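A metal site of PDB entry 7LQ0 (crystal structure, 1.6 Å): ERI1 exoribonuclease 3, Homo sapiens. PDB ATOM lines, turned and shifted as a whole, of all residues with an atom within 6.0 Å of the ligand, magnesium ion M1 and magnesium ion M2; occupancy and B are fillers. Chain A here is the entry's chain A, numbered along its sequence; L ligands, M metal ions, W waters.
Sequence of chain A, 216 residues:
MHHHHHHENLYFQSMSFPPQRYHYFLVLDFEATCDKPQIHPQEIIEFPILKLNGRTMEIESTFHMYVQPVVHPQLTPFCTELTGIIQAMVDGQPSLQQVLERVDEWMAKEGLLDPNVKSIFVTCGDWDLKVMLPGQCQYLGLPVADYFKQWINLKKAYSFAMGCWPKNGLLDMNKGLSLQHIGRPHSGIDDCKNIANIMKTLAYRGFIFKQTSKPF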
ATOM      1  N   ASP A  29       8.846  17.492  29.261  1.00  0.00           N
ATOM      2  CA  ASP A  29       9.774  18.627  29.245  1.00  0.00           C
ATOM      3  C   ASP A  29      11.137  18.077  28.827  1.00  0.00           C
ATOM      4  O   ASP A  29      11.833  17.480  29.650  1.00  0.00           O
ATOM      5  CB  ASP A  29       9.811  19.319  30.600  1.00  0.00           C
ATOM      6  CG  ASP A  29      10.232  20.807  30.512  1.00  0.00           C
ATOM      7  OD1 ASP A  29       9.659  21.680  31.221  1.00  0.00           O
ATOM      8  OD2 ASP A  29      11.167  21.111  29.790  1.00  0.00           O
ATOM      9  N   PHE A  30      11.472  18.196  27.540  1.00  0.00           N
ATOM     10  CA  PHE A  30      12.732  17.651  27.029  1.00  0.00           C
ATOM     11  C   PHE A  30      13.938  18.372  27.611  1.00  0.00           C
ATOM     12  O   PHE A  30      13.884  19.582  27.901  1.00  0.00           O
ATOM     13  CB  PHE A  30      12.832  17.786  25.498  1.00  0.00           C
ATOM     14  CG  PHE A  30      11.825  16.988  24.725  1.00  0.00           C
ATOM     15  CD1 PHE A  30      11.631  15.620  24.971  1.00  0.00           C
ATOM     16  CD2 PHE A  30      11.100  17.604  23.706  1.00  0.00           C
ATOM     17  CE1 PHE A  30      10.693  14.899  24.212  1.00  0.00           C
ATOM     18  CE2 PHE A  30      10.180  16.896  22.993  1.00  0.00           C
ATOM     19  CZ  PHE A  30      10.008  15.533  23.185  1.00  0.00           C
ATOM     20  N   GLU A  31      15.062  17.654  27.691  1.00  0.00           N
ATOM     21  CA  GLU A  31      16.348  18.324  27.562  1.00  0.00           C
ATOM     22  C   GLU A  31      16.989  17.930  26.242  1.00  0.00           C
ATOM     23  O   GLU A  31      16.711  16.862  25.694  1.00  0.00           O
ATOM     24  CB  GLU A  31      17.309  17.973  28.710  1.00  0.00           C
ATOM     25  CG  GLU A  31      16.766  18.291  30.100  1.00  0.00           C
ATOM     26  CD  GLU A  31      16.256  19.714  30.266  1.00  0.00           C
ATOM     27  OE1 GLU A  31      16.875  20.686  29.761  1.00  0.00           O
ATOM     28  OE2 GLU A  31      15.181  19.846  30.936  1.00  0.00           O
ATOM     29  N   ALA A  32      17.844  18.818  25.702  1.00  0.00           N
ATOM     30  CA  ALA A  32      18.467  18.585  24.408  1.00  0.00           C
ATOM     31  C   ALA A  32      19.923  18.999  24.456  1.00  0.00           C
ATOM     32  O   ALA A  32      20.332  19.789  25.310  1.00  0.00           O
ATOM     33  CB  ALA A  32      17.779  19.399  23.249  1.00  0.00           C
ATOM     34  N   THR A  33      20.718  18.465  23.528  1.00  0.00           N
ATOM     35  CA  THR A  33      22.077  18.986  23.395  1.00  0.00           C
ATOM     36  C   THR A  33      22.026  20.504  23.181  1.00  0.00           C
ATOM     37  O   THR A  33      21.048  21.055  22.660  1.00  0.00           O
ATOM     38  CB  THR A  33      22.805  18.351  22.195  1.00  0.00           C
ATOM     39  OG1 THR A  33      22.017  18.560  21.011  1.00  0.00           O
ATOM     40  CG2 THR A  33      23.014  16.829  22.400  1.00  0.00           C
ATOM     41  N   CYS A  34      23.100  21.190  23.554  1.00  0.00           N
ATOM     42  CA  CYS A  34      23.146  22.644  23.451  1.00  0.00           C
ATOM     43  C   CYS A  34      24.598  23.040  23.612  1.00  0.00           C
ATOM     44  O   CYS A  34      25.447  22.194  23.923  1.00  0.00           O
ATOM     45  CB  CYS A  34      22.259  23.335  24.502  1.00  0.00           C
ATOM     46  SG  CYS A  34      22.517  22.671  26.225  1.00  0.00           S
ATOM     47  N   ASP A  35      24.868  24.352  23.430  1.00  0.00           N
ATOM     48  CA  ASP A  35      26.197  24.908  23.492  1.00  0.00           C
ATOM     49  C   ASP A  35      26.037  26.422  23.483  1.00  0.00           C
ATOM     50  O   ASP A  35      24.920  26.942  23.311  1.00  0.00           O
ATOM     51  CB  ASP A  35      27.101  24.423  22.337  1.00  0.00           C
ATOM     52  CG  ASP A  35      28.602  24.522  22.683  1.00  0.00           C
ATOM     53  OD1 ASP A  35      28.909  24.998  23.802  1.00  0.00           O
ATOM     54  OD2 ASP A  35      29.465  24.103  21.843  1.00  0.00           O
ATOM     55  N   LYS A  36      27.157  27.123  23.650  1.00  0.00           N
ATOM     56  CA  LYS A  36      27.171  28.578  23.549  1.00  0.00           C
ATOM     57  C   LYS A  36      28.189  28.954  22.474  1.00  0.00           C
ATOM     58  O   LYS A  36      29.383  28.628  22.648  1.00  0.00           O
ATOM     59  CB  LYS A  36      27.563  29.161  24.907  1.00  0.00           C
ATOM     60  CG  LYS A  36      26.717  30.282  25.448  1.00  0.00           C
ATOM     61  CD  LYS A  36      25.331  29.791  25.721  1.00  0.00           C
ATOM     62  CE  LYS A  36      24.499  30.786  26.451  1.00  0.00           C
ATOM     63  NZ  LYS A  36      23.070  30.458  26.331  1.00  0.00           N
ATOM     64  N   GLN A  38      24.513  28.444  20.147  1.00  0.00           N
ATOM     65  CA  GLN A  38      23.722  27.220  20.206  1.00  0.00           C
ATOM     66  C   GLN A  38      24.235  26.179  19.227  1.00  0.00           C
ATOM     67  O   GLN A  38      24.682  26.500  18.101  1.00  0.00           O
ATOM     68  CB  GLN A  38      22.252  27.526  19.935  1.00  0.00           C
ATOM     69  CG  GLN A  38      21.301  26.338  20.172  1.00  0.00           C
ATOM     70  CD  GLN A  38      21.424  25.808  21.594  1.00  0.00           C
ATOM     71  OE1 GLN A  38      22.352  25.038  21.876  1.00  0.00           O
ATOM     72  NE2 GLN A  38      20.547  26.259  22.518  1.00  0.00           N
ATOM     73  N   GLN A  42      20.141  20.651  17.367  1.00  0.00           N
ATOM     74  CA  GLN A  42      19.930  20.121  18.711  1.00  0.00           C
ATOM     75  C   GLN A  42      19.306  18.754  18.626  1.00  0.00           C
ATOM     76  O   GLN A  42      18.636  18.418  17.651  1.00  0.00           O
ATOM     77  CB  GLN A  42      19.009  21.023  19.522  1.00  0.00           C
ATOM     78  CG  GLN A  42      19.621  22.398  19.833  1.00  0.00           C
ATOM     79  CD  GLN A  42      18.729  23.181  20.763  1.00  0.00           C
ATOM     80  OE1 GLN A  42      17.880  23.955  20.316  1.00  0.00           O
ATOM     81  NE2 GLN A  42      18.909  22.965  22.071  1.00  0.00           N
ATOM     82  N   ILE A  45      18.028  14.623  24.495  1.00  0.00           N
ATOM     83  CA  ILE A  45      18.826  13.715  25.327  1.00  0.00           C
ATOM     84  C   ILE A  45      18.081  13.240  26.573  1.00  0.00           C
ATOM     85  O   ILE A  45      18.580  12.343  27.261  1.00  0.00           O
ATOM     86  CB  ILE A  45      20.186  14.349  25.744  1.00  0.00           C
ATOM     87  CG1 ILE A  45      19.947  15.651  26.550  1.00  0.00           C
ATOM     88  CG2 ILE A  45      21.047  14.644  24.500  1.00  0.00           C
ATOM     89  CD1 ILE A  45      21.256  16.329  26.987  1.00  0.00           C
ATOM     90  N   PHE A  78      28.912  23.032  28.392  1.00  0.00           N
ATOM     91  CA  PHE A  78      27.726  23.833  28.660  1.00  0.00           C
ATOM     92  C   PHE A  78      26.479  22.968  28.869  1.00  0.00           C
ATOM     93  O   PHE A  78      25.705  23.194  29.792  1.00  0.00           O
ATOM     94  CB  PHE A  78      27.481  24.847  27.529  1.00  0.00           C
ATOM     95  CG  PHE A  78      26.243  25.649  27.757  1.00  0.00           C
ATOM     96  CD1 PHE A  78      26.273  26.753  28.634  1.00  0.00           C
ATOM     97  CD2 PHE A  78      25.035  25.255  27.212  1.00  0.00           C
ATOM     98  CE1 PHE A  78      25.130  27.465  28.904  1.00  0.00           C
ATOM     99  CE2 PHE A  78      23.861  25.949  27.494  1.00  0.00           C
ATOM    100  CZ  PHE A  78      23.906  27.081  28.336  1.00  0.00           C
ATOM    101  N   LEU A  82      24.329  22.982  32.219  1.00  0.00           N
ATOM    102  CA  LEU A  82      22.937  23.408  32.213  1.00  0.00           C
ATOM    103  C   LEU A  82      21.997  22.330  32.782  1.00  0.00           C
ATOM    104  O   LEU A  82      21.131  22.622  33.618  1.00  0.00           O
ATOM    105  CB  LEU A  82      22.497  23.745  30.797  1.00  0.00           C
ATOM    106  CG  LEU A  82      21.063  24.294  30.725  1.00  0.00           C
ATOM    107  CD1 LEU A  82      21.023  25.729  31.309  1.00  0.00           C
ATOM    108  CD2 LEU A  82      20.501  24.231  29.261  1.00  0.00           C
ATOM    109  N   THR A  83      22.105  21.105  32.270  1.00  0.00           N
ATOM    110  CA  THR A  83      21.112  20.057  32.514  1.00  0.00           C
ATOM    111  C   THR A  83      21.491  19.099  33.620  1.00  0.00           C
ATOM    112  O   THR A  83      20.607  18.363  34.106  1.00  0.00           O
ATOM    113  CB  THR A  83      20.886  19.215  31.262  1.00  0.00           C
ATOM    114  OG1 THR A  83      22.106  18.512  30.964  1.00  0.00           O
ATOM    115  CG2 THR A  83      20.473  20.133  30.061  1.00  0.00           C
ATOM    116  N   CYS A 124       5.782  23.262  29.034  1.00  0.00           N
ATOM    117  CA  CYS A 124       6.049  24.641  29.402  1.00  0.00           C
ATOM    118  C   CYS A 124       6.596  25.335  28.167  1.00  0.00           C
ATOM    119  O   CYS A 124       7.780  25.227  27.858  1.00  0.00           O
ATOM    120  CB  CYS A 124       7.047  24.700  30.554  1.00  0.00           C
ATOM    121  SG  CYS A 124       7.360  26.400  31.117  1.00  0.00           S
ATOM    122  N   TRP A 127       7.840  24.965  22.643  1.00  0.00           N
ATOM    123  CA  TRP A 127       9.046  24.541  21.934  1.00  0.00           C
ATOM    124  C   TRP A 127       9.111  23.018  21.779  1.00  0.00           C
ATOM    125  O   TRP A 127       9.501  22.491  20.723  1.00  0.00           O
ATOM    126  CB  TRP A 127      10.274  25.063  22.675  1.00  0.00           C
ATOM    127  CG  TRP A 127      11.597  24.645  22.081  1.00  0.00           C
ATOM    128  CD1 TRP A 127      12.233  25.183  20.956  1.00  0.00           C
ATOM    129  CD2 TRP A 127      12.450  23.621  22.569  1.00  0.00           C
ATOM    130  NE1 TRP A 127      13.434  24.549  20.745  1.00  0.00           N
ATOM    131  CE2 TRP A 127      13.582  23.565  21.701  1.00  0.00           C
ATOM    132  CE3 TRP A 127      12.386  22.743  23.662  1.00  0.00           C
ATOM    133  CZ2 TRP A 127      14.641  22.696  21.923  1.00  0.00           C
ATOM    134  CZ3 TRP A 127      13.446  21.837  23.858  1.00  0.00           C
ATOM    135  CH2 TRP A 127      14.543  21.820  22.981  1.00  0.00           C
ATOM    136  N   ASP A 128       8.805  22.293  22.846  1.00  0.00           N
ATOM    137  CA  ASP A 128       9.054  20.849  22.834  1.00  0.00           C
ATOM    138  C   ASP A 128       8.361  20.137  21.687  1.00  0.00           C
ATOM    139  O   ASP A 128       8.988  19.338  20.967  1.00  0.00           O
ATOM    140  CB  ASP A 128       8.587  20.241  24.165  1.00  0.00           C
ATOM    141  CG  ASP A 128       9.289  20.859  25.328  1.00  0.00           C
ATOM    142  OD1 ASP A 128      10.088  20.183  25.979  1.00  0.00           O
ATOM    143  OD2 ASP A 128       9.046  22.053  25.593  1.00  0.00           O
ATOM    144  N   PRO A 185      16.206  23.044  38.333  1.00  0.00           N
ATOM    145  CA  PRO A 185      15.796  23.560  36.994  1.00  0.00           C
ATOM    146  C   PRO A 185      16.627  22.928  35.883  1.00  0.00           C
ATOM    147  O   PRO A 185      17.813  22.651  36.064  1.00  0.00           O
ATOM    148  CB  PRO A 185      16.073  25.074  37.106  1.00  0.00           C
ATOM    149  CG  PRO A 185      15.926  25.317  38.621  1.00  0.00           C
ATOM    150  CD  PRO A 185      16.510  24.136  39.287  1.00  0.00           C
ATOM    151  N   HIS A 186      15.994  22.676  34.745  1.00  0.00           N
ATOM    152  CA  HIS A 186      16.647  22.104  33.559  1.00  0.00           C
ATOM    153  C   HIS A 186      17.021  20.627  33.697  1.00  0.00           C
ATOM    154  O   HIS A 186      17.784  20.097  32.862  1.00  0.00           O
ATOM    155  CB  HIS A 186      17.891  22.911  33.180  1.00  0.00           C
ATOM    156  CG  HIS A 186      17.614  24.364  33.038  1.00  0.00           C
ATOM    157  ND1 HIS A 186      16.864  24.882  32.006  1.00  0.00           N
ATOM    158  CD2 HIS A 186      17.977  25.424  33.804  1.00  0.00           C
ATOM    159  CE1 HIS A 186      16.780  26.190  32.141  1.00  0.00           C
ATOM    160  NE2 HIS A 186      17.453  26.548  33.223  1.00  0.00           N
ATOM    161  N   SER A 187      16.506  19.928  34.710  1.00  0.00           N
ATOM    162  CA  SER A 187      16.404  18.480  34.698  1.00  0.00           C
ATOM    163  C   SER A 187      15.015  18.190  34.160  1.00  0.00           C
ATOM    164  O   SER A 187      14.047  18.770  34.647  1.00  0.00           O
ATOM    165  CB  SER A 187      16.559  17.895  36.102  1.00  0.00           C
ATOM    166  OG  SER A 187      15.998  16.589  36.109  1.00  0.00           O
ATOM    167  N   GLY A 188      14.936  17.365  33.108  1.00  0.00           N
ATOM    168  CA  GLY A 188      13.654  17.191  32.446  1.00  0.00           C
ATOM    169  C   GLY A 188      12.618  16.623  33.395  1.00  0.00           C
ATOM    170  O   GLY A 188      11.493  17.127  33.488  1.00  0.00           O
ATOM    171  N   ASP A 191      11.648  19.321  35.910  1.00  0.00           N
ATOM    172  CA  ASP A 191      10.793  20.320  35.271  1.00  0.00           C
ATOM    173  C   ASP A 191       9.369  19.772  35.164  1.00  0.00           C
ATOM    174  O   ASP A 191       8.401  20.497  35.433  1.00  0.00           O
ATOM    175  CB  ASP A 191      11.337  20.656  33.897  1.00  0.00           C
ATOM    176  CG  ASP A 191      12.534  21.619  33.937  1.00  0.00           C
ATOM    177  OD1 ASP A 191      12.884  22.163  35.009  1.00  0.00           O
ATOM    178  OD2 ASP A 191      13.130  21.838  32.852  1.00  0.00           O
HETATM  179  P1  LIG L   1      14.700  23.668  29.459  1.00  0.00           P
HETATM  180  O1  LIG L   1      13.436  22.800  29.430  1.00  0.00           O
HETATM  181  O2  LIG L   1      15.808  22.903  30.215  1.00  0.00           O
HETATM  182  O3  LIG L   1      14.562  25.042  30.058  1.00  0.00           O
HETATM  183  O4  LIG L   1      15.255  23.852  27.993  1.00  0.00           O
HETATM  184  C1  LIG L   1      15.205  22.841  27.015  1.00  0.00           C
HETATM  185  C2  LIG L   1      16.508  22.822  26.237  1.00  0.00           C
HETATM  186  O5  LIG L   1      16.746  24.136  25.657  1.00  0.00           O
HETATM  187  C3  LIG L   1      17.759  22.562  27.062  1.00  0.00           C
HETATM  188  O6  LIG L   1      17.994  21.162  27.304  1.00  0.00           O
HETATM  189  C4  LIG L   1      18.843  23.180  26.183  1.00  0.00           C
HETATM  190  O7  LIG L   1      19.093  22.318  25.076  1.00  0.00           O
HETATM  191  C5  LIG L   1      18.123  24.435  25.660  1.00  0.00           C
HETATM  192  N1  LIG L   1      18.342  25.590  26.542  1.00  0.00           N
HETATM  193  C6  LIG L   1      17.619  25.875  27.660  1.00  0.00           C
HETATM  194  N2  LIG L   1      18.130  26.989  28.291  1.00  0.00           N
HETATM  195  C7  LIG L   1      19.202  27.368  27.559  1.00  0.00           C
HETATM  196  C8  LIG L   1      20.180  28.455  27.666  1.00  0.00           C
HETATM  197  N3  LIG L   1      20.072  29.341  28.686  1.00  0.00           N
HETATM  198  N4  LIG L   1      21.153  28.508  26.750  1.00  0.00           N
HETATM  199  C9  LIG L   1      21.250  27.590  25.754  1.00  0.00           C
HETATM  200  N5  LIG L   1      20.380  26.572  25.585  1.00  0.00           N
HETATM  201  C10 LIG L   1      19.356  26.449  26.453  1.00  0.00           C
HETATM  202 MG    MG M   1      13.376  20.983  30.825  1.00  0.00          MG
HETATM  203 MG    MG M   2      11.546  22.885  28.692  1.00  0.00          MG
HETATM  204  O   HOH W   1      17.850  29.178  30.712  1.00  0.00           O
HETATM  205  O   HOH W   2      12.083  21.514  27.180  1.00  0.00           O
HETATM  206  O   HOH W   3      13.800  27.594  29.946  1.00  0.00           O
HETATM  207  O   HOH W   4      13.210  24.638  32.360  1.00  0.00           O
HETATM  208  O   HOH W   5      10.822  23.891  30.329  1.00  0.00           O
HETATM  209  O   HOH W   6      12.176  24.582  27.675  1.00  0.00           O
HETATM  210  O   HOH W   7      16.963  25.571  22.696  1.00  0.00           O
HETATM  211  O   HOH W   8       9.698  23.125  27.731  1.00  0.00           O
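NE2 of Gln 42 is in hydrogen-bond range of O7 of the ligand, at 3.1 Å. ND1 of His 186 sits at hydrogen-bond distance from O2 of the ligand (2.9 Å). The backbone carbonyl oxygen (O) of Ala 32 lies within hydrogen-bond range of an oxygen (O7) of the ligand, 2.8 Å away. N4 of the ligand sits at hydrogen-bond distance from NZ of Lys 36. NE2 of Gln 38 lies within hydrogen-bond range of N5 of the ligand (3.1 Å). An oxygen (O7) of the ligand is in hydrogen-bond range of the backbone carbonyl oxygen (O) of Thr 33, at 3.4 Å. The backbone NH of Ala 32 sits at hydrogen-bond distance from an oxygen (O6) of the ligand, at 2.8 Å. An oxygen (O7) of the ligand sits close to the side-chain sulfur (SG) of Cys 34.
The side-chain amide oxygen of Gln 38 lies within hydrogen-bond range of the backbone NH of Asp 35 (3.0 Å). The side-chain carboxylate (OD1) of Asp 191 sits at hydrogen-bond distance from the backbone NH (N) of His 186 (3.2 Å). The side-chain carboxylate (OE2) of Glu 31 sits close to the backbone NH (N) of Gly 188 (3.3 Å). N of Phe 30 lies within hydrogen-bond range of OD1 of Asp 128. O of Glu 31 is in hydrogen-bond range of N of Ile 45. The side-chain amide nitrogen (NE2) of Gln 42 sits at hydrogen-bond distance from the backbone carbonyl oxygen (O) of Thr 33 (2.9 Å). The backbone carbonyl oxygen of Ala 32 lies within hydrogen-bond range of the side-chain sulfur of Cys 34, at 3.7 Å.
Residues that only touch the ligand: Phe 78 (3.5 Å), Phe 30 (3.6 Å), Leu 82 (3.7 Å), Trp 127 (3.8 Å) and Thr 83 (3.8 Å). Hydrophobic or aromatic side chains within 4 Å of the ligand: Ala 32, Phe 78, Leu 82, Trp 127 and His 186. Within 4 Å of the ligand: Asp 29, Phe 30, Glu 31, Ala 32, Thr 33, Cys 34, Lys 36, Gln 38, Gln 42, Phe 78, Leu 82, Thr 83, Trp 127, His 186 and Asp 191. The nearest printed residue that does not touch the ligand is Asp 35 (4.5 Å).
Merely in contact with magnesium ion M1: Phe 30. Four residues have an atom within 4 Å of magnesium ion M1: Asp 29, Phe 30, Glu 31 and Asp 191. The nearest printed residue that does not touch magnesium ion M1 is Gly 188 (4.1 Å).
One residue has an atom within 4 Å of magnesium ion M2: Asp 29. The nearest printed residue that does not touch magnesium ion M2 is Asp 128 (4.1 Å).
OE2 of Glu 31 binds magnesium ion M1, 2.1 Å away. OD2 of Asp 191 binds magnesium ion M1 (2.2 Å). An oxygen (O1) of the ligand is bound to magnesium ion M1, at 2.3 Å. The side-chain carboxylate (OD2) of Asp 29 binds magnesium ion M1 (2.4 Å).
Magnesium ion M2 is bound by O1 of the ligand (2.0 Å). Water W5 binds magnesium ion M2, 2.1 Å away. Water W6 binds magnesium ion M2 (2.1 Å). Water W8 is bound to magnesium ion M2 (2.1 Å). Water W2 is bound to magnesium ion M2, 2.1 Å away. OD2 of Asp 29 binds magnesium ion M2, at 2.1 Å.
Water W2 lies within hydrogen-bond range of the side-chain carboxylate (OD1) of Asp 128 and the backbone carbonyl oxygen (O) of Phe 30. Water W8 lies within hydrogen-bond range of OD2 of Asp 128 and O of Cys 124. Water W7 bridges OE1 of Gln 42 and O5 of the ligand.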
